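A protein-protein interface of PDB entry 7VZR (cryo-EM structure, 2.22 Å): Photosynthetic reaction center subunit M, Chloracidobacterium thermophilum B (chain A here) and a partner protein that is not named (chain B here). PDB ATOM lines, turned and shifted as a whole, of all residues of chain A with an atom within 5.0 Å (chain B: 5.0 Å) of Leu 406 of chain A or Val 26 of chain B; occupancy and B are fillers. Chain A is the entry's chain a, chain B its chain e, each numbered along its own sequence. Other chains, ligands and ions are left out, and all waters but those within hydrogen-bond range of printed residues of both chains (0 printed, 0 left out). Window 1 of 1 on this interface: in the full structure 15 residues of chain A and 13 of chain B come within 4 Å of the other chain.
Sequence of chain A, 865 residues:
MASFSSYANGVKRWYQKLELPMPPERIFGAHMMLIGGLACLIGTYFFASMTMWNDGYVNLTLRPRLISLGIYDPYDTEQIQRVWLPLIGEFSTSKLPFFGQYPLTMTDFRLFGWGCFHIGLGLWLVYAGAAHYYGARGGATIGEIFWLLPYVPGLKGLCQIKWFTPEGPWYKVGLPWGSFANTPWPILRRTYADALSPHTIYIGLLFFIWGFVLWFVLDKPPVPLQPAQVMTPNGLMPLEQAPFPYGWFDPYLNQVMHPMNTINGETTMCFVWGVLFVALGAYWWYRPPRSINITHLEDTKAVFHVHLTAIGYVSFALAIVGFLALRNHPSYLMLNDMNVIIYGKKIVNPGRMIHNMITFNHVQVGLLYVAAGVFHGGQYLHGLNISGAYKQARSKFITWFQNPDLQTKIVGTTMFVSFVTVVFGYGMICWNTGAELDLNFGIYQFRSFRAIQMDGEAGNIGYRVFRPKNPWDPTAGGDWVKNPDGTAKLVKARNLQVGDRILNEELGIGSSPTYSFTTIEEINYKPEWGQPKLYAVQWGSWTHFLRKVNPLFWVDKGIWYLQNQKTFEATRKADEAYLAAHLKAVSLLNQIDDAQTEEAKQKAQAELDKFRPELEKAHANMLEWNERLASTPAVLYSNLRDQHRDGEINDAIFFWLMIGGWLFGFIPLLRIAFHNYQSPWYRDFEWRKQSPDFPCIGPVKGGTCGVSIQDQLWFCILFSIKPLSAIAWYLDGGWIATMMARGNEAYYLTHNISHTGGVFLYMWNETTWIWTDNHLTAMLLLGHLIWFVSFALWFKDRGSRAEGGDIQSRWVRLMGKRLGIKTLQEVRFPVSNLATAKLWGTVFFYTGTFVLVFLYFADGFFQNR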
ATOM      1  N   TRP A 400     -25.655 -23.751 -30.016  1.00  0.00           N
ATOM      2  CA  TRP A 400     -25.632 -23.534 -28.585  1.00  0.00           C
ATOM      3  C   TRP A 400     -26.237 -24.657 -27.811  1.00  0.00           C
ATOM      4  O   TRP A 400     -25.966 -24.771 -26.643  1.00  0.00           O
ATOM      5  CB  TRP A 400     -26.424 -22.318 -28.148  1.00  0.00           C
ATOM      6  CG  TRP A 400     -25.819 -21.031 -28.170  1.00  0.00           C
ATOM      7  CD1 TRP A 400     -24.517 -20.712 -28.125  1.00  0.00           C
ATOM      8  CD2 TRP A 400     -26.522 -19.830 -28.237  1.00  0.00           C
ATOM      9  NE1 TRP A 400     -24.377 -19.392 -28.175  1.00  0.00           N
ATOM     10  CE2 TRP A 400     -25.604 -18.820 -28.253  1.00  0.00           C
ATOM     11  CE3 TRP A 400     -27.867 -19.520 -28.337  1.00  0.00           C
ATOM     12  CZ2 TRP A 400     -25.974 -17.523 -28.321  1.00  0.00           C
ATOM     13  CZ3 TRP A 400     -28.218 -18.273 -28.402  1.00  0.00           C
ATOM     14  CH2 TRP A 400     -27.288 -17.274 -28.398  1.00  0.00           C
ATOM     15  N   PHE A 401     -27.072 -25.462 -28.408  1.00  0.00           N
ATOM     16  CA  PHE A 401     -27.738 -26.526 -27.707  1.00  0.00           C
ATOM     17  C   PHE A 401     -27.466 -27.912 -28.264  1.00  0.00           C
ATOM     18  O   PHE A 401     -28.276 -28.775 -28.057  1.00  0.00           O
ATOM     19  CB  PHE A 401     -29.231 -26.314 -27.737  1.00  0.00           C
ATOM     20  CG  PHE A 401     -29.679 -25.033 -27.208  1.00  0.00           C
ATOM     21  CD1 PHE A 401     -29.915 -24.852 -25.877  1.00  0.00           C
ATOM     22  CD2 PHE A 401     -29.873 -23.992 -28.043  1.00  0.00           C
ATOM     23  CE1 PHE A 401     -30.319 -23.653 -25.438  1.00  0.00           C
ATOM     24  CE2 PHE A 401     -30.271 -22.842 -27.608  1.00  0.00           C
ATOM     25  CZ  PHE A 401     -30.498 -22.653 -26.329  1.00  0.00           C
ATOM     26  N   ASN A 403     -24.757 -30.075 -27.640  1.00  0.00           N
ATOM     27  CA  ASN A 403     -24.171 -30.985 -26.681  1.00  0.00           C
ATOM     28  C   ASN A 403     -25.258 -31.761 -25.913  1.00  0.00           C
ATOM     29  O   ASN A 403     -26.117 -31.144 -25.300  1.00  0.00           O
ATOM     30  CB  ASN A 403     -23.302 -30.148 -25.767  1.00  0.00           C
ATOM     31  CG  ASN A 403     -22.514 -30.944 -24.810  1.00  0.00           C
ATOM     32  OD1 ASN A 403     -22.947 -31.256 -23.751  1.00  0.00           O
ATOM     33  ND2 ASN A 403     -21.344 -31.299 -25.199  1.00  0.00           N
ATOM     34  N   PRO A 404     -25.272 -33.094 -25.963  1.00  0.00           N
ATOM     35  CA  PRO A 404     -26.365 -33.829 -25.320  1.00  0.00           C
ATOM     36  C   PRO A 404     -26.346 -33.763 -23.819  1.00  0.00           C
ATOM     37  O   PRO A 404     -27.400 -33.937 -23.207  1.00  0.00           O
ATOM     38  CB  PRO A 404     -26.138 -35.261 -25.794  1.00  0.00           C
ATOM     39  CG  PRO A 404     -25.385 -35.133 -26.972  1.00  0.00           C
ATOM     40  CD  PRO A 404     -24.494 -33.983 -26.817  1.00  0.00           C
ATOM     41  N   ASP A 405     -25.202 -33.472 -23.217  1.00  0.00           N
ATOM     42  CA  ASP A 405     -25.089 -33.445 -21.776  1.00  0.00           C
ATOM     43  C   ASP A 405     -25.626 -32.139 -21.205  1.00  0.00           C
ATOM     44  O   ASP A 405     -26.383 -32.157 -20.242  1.00  0.00           O
ATOM     45  CB  ASP A 405     -23.628 -33.686 -21.443  1.00  0.00           C
ATOM     46  CG  ASP A 405     -23.310 -33.583 -20.004  1.00  0.00           C
ATOM     47  OD1 ASP A 405     -23.880 -34.304 -19.172  1.00  0.00           O
ATOM     48  OD2 ASP A 405     -22.424 -32.779 -19.684  1.00  0.00           O
ATOM     49  N   LEU A 406     -25.307 -31.003 -21.827  1.00  0.00           N
ATOM     50  CA  LEU A 406     -26.059 -29.794 -21.571  1.00  0.00           C
ATOM     51  C   LEU A 406     -27.569 -30.007 -21.740  1.00  0.00           C
ATOM     52  O   LEU A 406     -28.336 -29.541 -20.926  1.00  0.00           O
ATOM     53  CB  LEU A 406     -25.552 -28.645 -22.435  1.00  0.00           C
ATOM     54  CG  LEU A 406     -26.247 -27.265 -22.410  1.00  0.00           C
ATOM     55  CD1 LEU A 406     -25.954 -26.436 -21.261  1.00  0.00           C
ATOM     56  CD2 LEU A 406     -26.071 -26.472 -23.581  1.00  0.00           C
ATOM     57  N   GLN A 407     -28.021 -30.745 -22.747  1.00  0.00           N
ATOM     58  CA  GLN A 407     -29.456 -30.941 -22.896  1.00  0.00           C
ATOM     59  C   GLN A 407     -30.052 -31.676 -21.688  1.00  0.00           C
ATOM     60  O   GLN A 407     -31.056 -31.229 -21.131  1.00  0.00           O
ATOM     61  CB  GLN A 407     -29.787 -31.659 -24.213  1.00  0.00           C
ATOM     62  CG  GLN A 407     -29.407 -30.980 -25.479  1.00  0.00           C
ATOM     63  CD  GLN A 407     -29.546 -31.847 -26.662  1.00  0.00           C
ATOM     64  OE1 GLN A 407     -29.739 -32.988 -26.524  1.00  0.00           O
ATOM     65  NE2 GLN A 407     -29.485 -31.297 -27.820  1.00  0.00           N
ATOM     66  N   THR A 408     -29.388 -32.723 -21.173  1.00  0.00           N
ATOM     67  CA  THR A 408     -29.931 -33.340 -19.949  1.00  0.00           C
ATOM     68  C   THR A 408     -29.781 -32.446 -18.713  1.00  0.00           C
ATOM     69  O   THR A 408     -30.688 -32.405 -17.900  1.00  0.00           O
ATOM     70  CB  THR A 408     -29.423 -34.799 -19.754  1.00  0.00           C
ATOM     71  OG1 THR A 408     -29.308 -35.231 -18.390  1.00  0.00           O
ATOM     72  CG2 THR A 408     -28.267 -35.084 -20.437  1.00  0.00           C
ATOM     73  N   LYS A 409     -28.746 -31.636 -18.601  1.00  0.00           N
ATOM     74  CA  LYS A 409     -28.699 -30.703 -17.481  1.00  0.00           C
ATOM     75  C   LYS A 409     -29.834 -29.676 -17.531  1.00  0.00           C
ATOM     76  O   LYS A 409     -30.530 -29.515 -16.551  1.00  0.00           O
ATOM     77  CB  LYS A 409     -27.350 -30.030 -17.360  1.00  0.00           C
ATOM     78  CG  LYS A 409     -26.310 -30.885 -16.708  1.00  0.00           C
ATOM     79  CD  LYS A 409     -24.920 -30.544 -17.015  1.00  0.00           C
ATOM     80  CE  LYS A 409     -23.983 -31.593 -16.571  1.00  0.00           C
ATOM     81  NZ  LYS A 409     -22.627 -31.145 -16.600  1.00  0.00           N
ATOM     82  N   ILE A 410     -30.082 -29.037 -18.664  1.00  0.00           N
ATOM     83  CA  ILE A 410     -31.190 -28.099 -18.799  1.00  0.00           C
ATOM     84  C   ILE A 410     -32.510 -28.733 -18.378  1.00  0.00           C
ATOM     85  O   ILE A 410     -33.214 -28.210 -17.511  1.00  0.00           O
ATOM     86  CB  ILE A 410     -31.275 -27.562 -20.230  1.00  0.00           C
ATOM     87  CG1 ILE A 410     -30.133 -26.609 -20.562  1.00  0.00           C
ATOM     88  CG2 ILE A 410     -32.539 -26.884 -20.390  1.00  0.00           C
ATOM     89  CD1 ILE A 410     -29.914 -26.371 -21.963  1.00  0.00           C
ATOM     90  N   VAL A 411     -32.854 -29.867 -18.983  1.00  0.00           N
ATOM     91  CA  VAL A 411     -34.142 -30.499 -18.744  1.00  0.00           C
ATOM     92  C   VAL A 411     -34.297 -30.950 -17.308  1.00  0.00           C
ATOM     93  O   VAL A 411     -35.351 -30.743 -16.715  1.00  0.00           O
ATOM     94  CB  VAL A 411     -34.382 -31.682 -19.697  1.00  0.00           C
ATOM     95  CG1 VAL A 411     -35.652 -32.302 -19.403  1.00  0.00           C
ATOM     96  CG2 VAL A 411     -34.405 -31.254 -21.055  1.00  0.00           C
ATOM     97  N   ILE B  22     -30.363 -22.730 -14.079  1.00  0.00           N
ATOM     98  CA  ILE B  22     -29.928 -23.598 -15.112  1.00  0.00           C
ATOM     99  C   ILE B  22     -28.578 -23.225 -15.567  1.00  0.00           C
ATOM    100  O   ILE B  22     -28.035 -23.882 -16.347  1.00  0.00           O
ATOM    101  CB  ILE B  22     -30.959 -23.568 -16.200  1.00  0.00           C
ATOM    102  CG1 ILE B  22     -31.964 -24.599 -15.937  1.00  0.00           C
ATOM    103  CG2 ILE B  22     -30.433 -23.980 -17.510  1.00  0.00           C
ATOM    104  CD1 ILE B  22     -32.953 -24.564 -17.028  1.00  0.00           C
ATOM    105  N   LYS B  23     -27.986 -22.197 -15.033  1.00  0.00           N
ATOM    106  CA  LYS B  23     -26.663 -21.838 -15.428  1.00  0.00           C
ATOM    107  C   LYS B  23     -25.788 -21.763 -14.223  1.00  0.00           C
ATOM    108  O   LYS B  23     -24.751 -21.213 -14.269  1.00  0.00           O
ATOM    109  CB  LYS B  23     -26.746 -20.512 -16.085  1.00  0.00           C
ATOM    110  CG  LYS B  23     -25.463 -19.931 -16.523  1.00  0.00           C
ATOM    111  CD  LYS B  23     -25.765 -18.677 -17.280  1.00  0.00           C
ATOM    112  CE  LYS B  23     -24.633 -17.697 -17.141  1.00  0.00           C
ATOM    113  NZ  LYS B  23     -23.978 -17.527 -18.460  1.00  0.00           N
ATOM    114  N   PHE B  24     -26.209 -22.310 -13.108  1.00  0.00           N
ATOM    115  CA  PHE B  24     -25.424 -22.264 -11.935  1.00  0.00           C
ATOM    116  C   PHE B  24     -25.140 -23.687 -11.858  1.00  0.00           C
ATOM    117  O   PHE B  24     -24.180 -24.089 -11.315  1.00  0.00           O
ATOM    118  CB  PHE B  24     -26.260 -21.863 -10.760  1.00  0.00           C
ATOM    119  CG  PHE B  24     -25.615 -22.125  -9.446  1.00  0.00           C
ATOM    120  CD1 PHE B  24     -24.674 -21.287  -8.963  1.00  0.00           C
ATOM    121  CD2 PHE B  24     -25.962 -23.197  -8.708  1.00  0.00           C
ATOM    122  CE1 PHE B  24     -24.071 -21.518  -7.772  1.00  0.00           C
ATOM    123  CE2 PHE B  24     -25.369 -23.441  -7.515  1.00  0.00           C
ATOM    124  CZ  PHE B  24     -24.424 -22.598  -7.049  1.00  0.00           C
ATOM    125  N   VAL B  25     -26.019 -24.466 -12.415  1.00  0.00           N
ATOM    126  CA  VAL B  25     -25.833 -25.939 -12.501  1.00  0.00           C
ATOM    127  C   VAL B  25     -24.821 -26.285 -13.602  1.00  0.00           C
ATOM    128  O   VAL B  25     -24.126 -27.253 -13.397  1.00  0.00           O
ATOM    129  CB  VAL B  25     -27.156 -26.722 -12.631  1.00  0.00           C
ATOM    130  CG1 VAL B  25     -26.930 -28.160 -13.054  1.00  0.00           C
ATOM    131  CG2 VAL B  25     -28.003 -26.646 -11.373  1.00  0.00           C
ATOM    132  N   VAL B  26     -24.849 -25.648 -14.718  1.00  0.00           N
ATOM    133  CA  VAL B  26     -23.974 -25.887 -15.763  1.00  0.00           C
ATOM    134  C   VAL B  26     -22.630 -25.451 -15.436  1.00  0.00           C
ATOM    135  O   VAL B  26     -21.784 -26.173 -15.593  1.00  0.00           O
ATOM    136  CB  VAL B  26     -24.466 -25.308 -17.035  1.00  0.00           C
ATOM    137  CG1 VAL B  26     -23.385 -25.284 -18.062  1.00  0.00           C
ATOM    138  CG2 VAL B  26     -25.546 -26.203 -17.461  1.00  0.00           C
ATOM    139  N   ALA B  27     -22.463 -24.310 -14.841  1.00  0.00           N
ATOM    140  CA  ALA B  27     -21.177 -23.859 -14.479  1.00  0.00           C
ATOM    141  C   ALA B  27     -20.549 -24.634 -13.379  1.00  0.00           C
ATOM    142  O   ALA B  27     -19.391 -24.682 -13.353  1.00  0.00           O
ATOM    143  CB  ALA B  27     -21.181 -22.428 -14.140  1.00  0.00           C
ATOM    144  N   ASN B  28     -21.286 -25.180 -12.426  1.00  0.00           N
ATOM    145  CA  ASN B  28     -20.607 -25.923 -11.414  1.00  0.00           C
ATOM    146  C   ASN B  28     -20.668 -27.390 -11.392  1.00  0.00           C
ATOM    147  O   ASN B  28     -20.383 -27.937 -10.482  1.00  0.00           O
ATOM    148  CB  ASN B  28     -20.385 -25.237 -10.060  1.00  0.00           C
ATOM    149  CG  ASN B  28     -21.467 -24.431  -9.639  1.00  0.00           C
ATOM    150  OD1 ASN B  28     -21.512 -23.281  -9.845  1.00  0.00           O
ATOM    151  ND2 ASN B  28     -22.352 -25.042  -9.040  1.00  0.00           N
ATOM    152  N   THR B  29     -21.039 -27.992 -12.492  1.00  0.00           N
ATOM    153  CA  THR B  29     -20.972 -29.369 -12.623  1.00  0.00           C
ATOM    154  C   THR B  29     -20.273 -29.573 -13.911  1.00  0.00           C
ATOM    155  O   THR B  29     -20.605 -30.451 -14.619  1.00  0.00           O
ATOM    156  CB  THR B  29     -22.351 -30.108 -12.673  1.00  0.00           C
ATOM    157  OG1 THR B  29     -23.166 -29.589 -13.686  1.00  0.00           O
ATOM    158  CG2 THR B  29     -23.108 -30.048 -11.447  1.00  0.00           C
ATOM    159  N   LYS B  30     -19.278 -28.788 -14.257  1.00  0.00           N
ATOM    160  CA  LYS B  30     -18.663 -29.015 -15.526  1.00  0.00           C
ATOM    161  C   LYS B  30     -17.634 -30.097 -15.638  1.00  0.00           C
ATOM    162  O   LYS B  30     -17.269 -30.507 -16.678  1.00  0.00           O
ATOM    163  CB  LYS B  30     -18.471 -27.791 -16.321  1.00  0.00           C
ATOM    164  CG  LYS B  30     -17.086 -27.434 -16.487  1.00  0.00           C
ATOM    165  CD  LYS B  30     -17.028 -26.093 -15.891  1.00  0.00           C
ATOM    166  CE  LYS B  30     -16.618 -25.120 -16.957  1.00  0.00           C
ATOM    167  NZ  LYS B  30     -15.224 -24.701 -16.669  1.00  0.00           N
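The side-chain amino group of Lys 409 of chain A sits at hydrogen-bond distance from the backbone carbonyl oxygen of Thr 29 of chain B (2.9 Å).
The backbone NH (N) of Leu 406 of chain A lies within hydrogen-bond range of the side-chain amide oxygen (OD1) of Asn 403 of chain A. The side-chain carboxylate (OD2) of Asp 405 of chain A is in salt-bridge range of the side-chain amino group (NZ) of Lys 409 of chain A. The backbone carbonyl oxygen of Val 25 of chain B lies within hydrogen-bond range of the side-chain hydroxyl of Thr 29 of chain B.
Among the printed residues, pairs that only touch across the chains: Leu 406 of chain A with Val 26 of chain B (3.8 Å) and Ile 410 of chain A with Ile 22 of chain B (3.7 Å).
Leu 406 of chain A touches one residue of chain B. Of the printed residues of chain B, Lys 409 of chain A touches Thr 29. Of the printed residues of chain A, Ile 22 of chain B touches Ile 410. Of chain A, only Leu 406 comes within 4 Å of Val 26 of chain B. The nearest residue of chain A that does not touch Val 26 of chain B is Lys 409 of chain A (4.2 Å). The nearest printed residue of chain B that does not touch Ile 410 of chain A is Val 26 of chain B (5.5 Å).
Of the 9 printed residues of chain B, 3 touch a printed residue of chain A. Printed residues of chain A that touch a printed residue of chain B: Leu 406, Lys 409 and Ile 410. Hydrophobic or aromatic side chains of chain A that line the printed part of chain B: Leu 406. Among the printed residues, no Asp or Glu carboxylate lies within 4 Å of a Lys or Arg side-chain nitrogen of the other chain.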
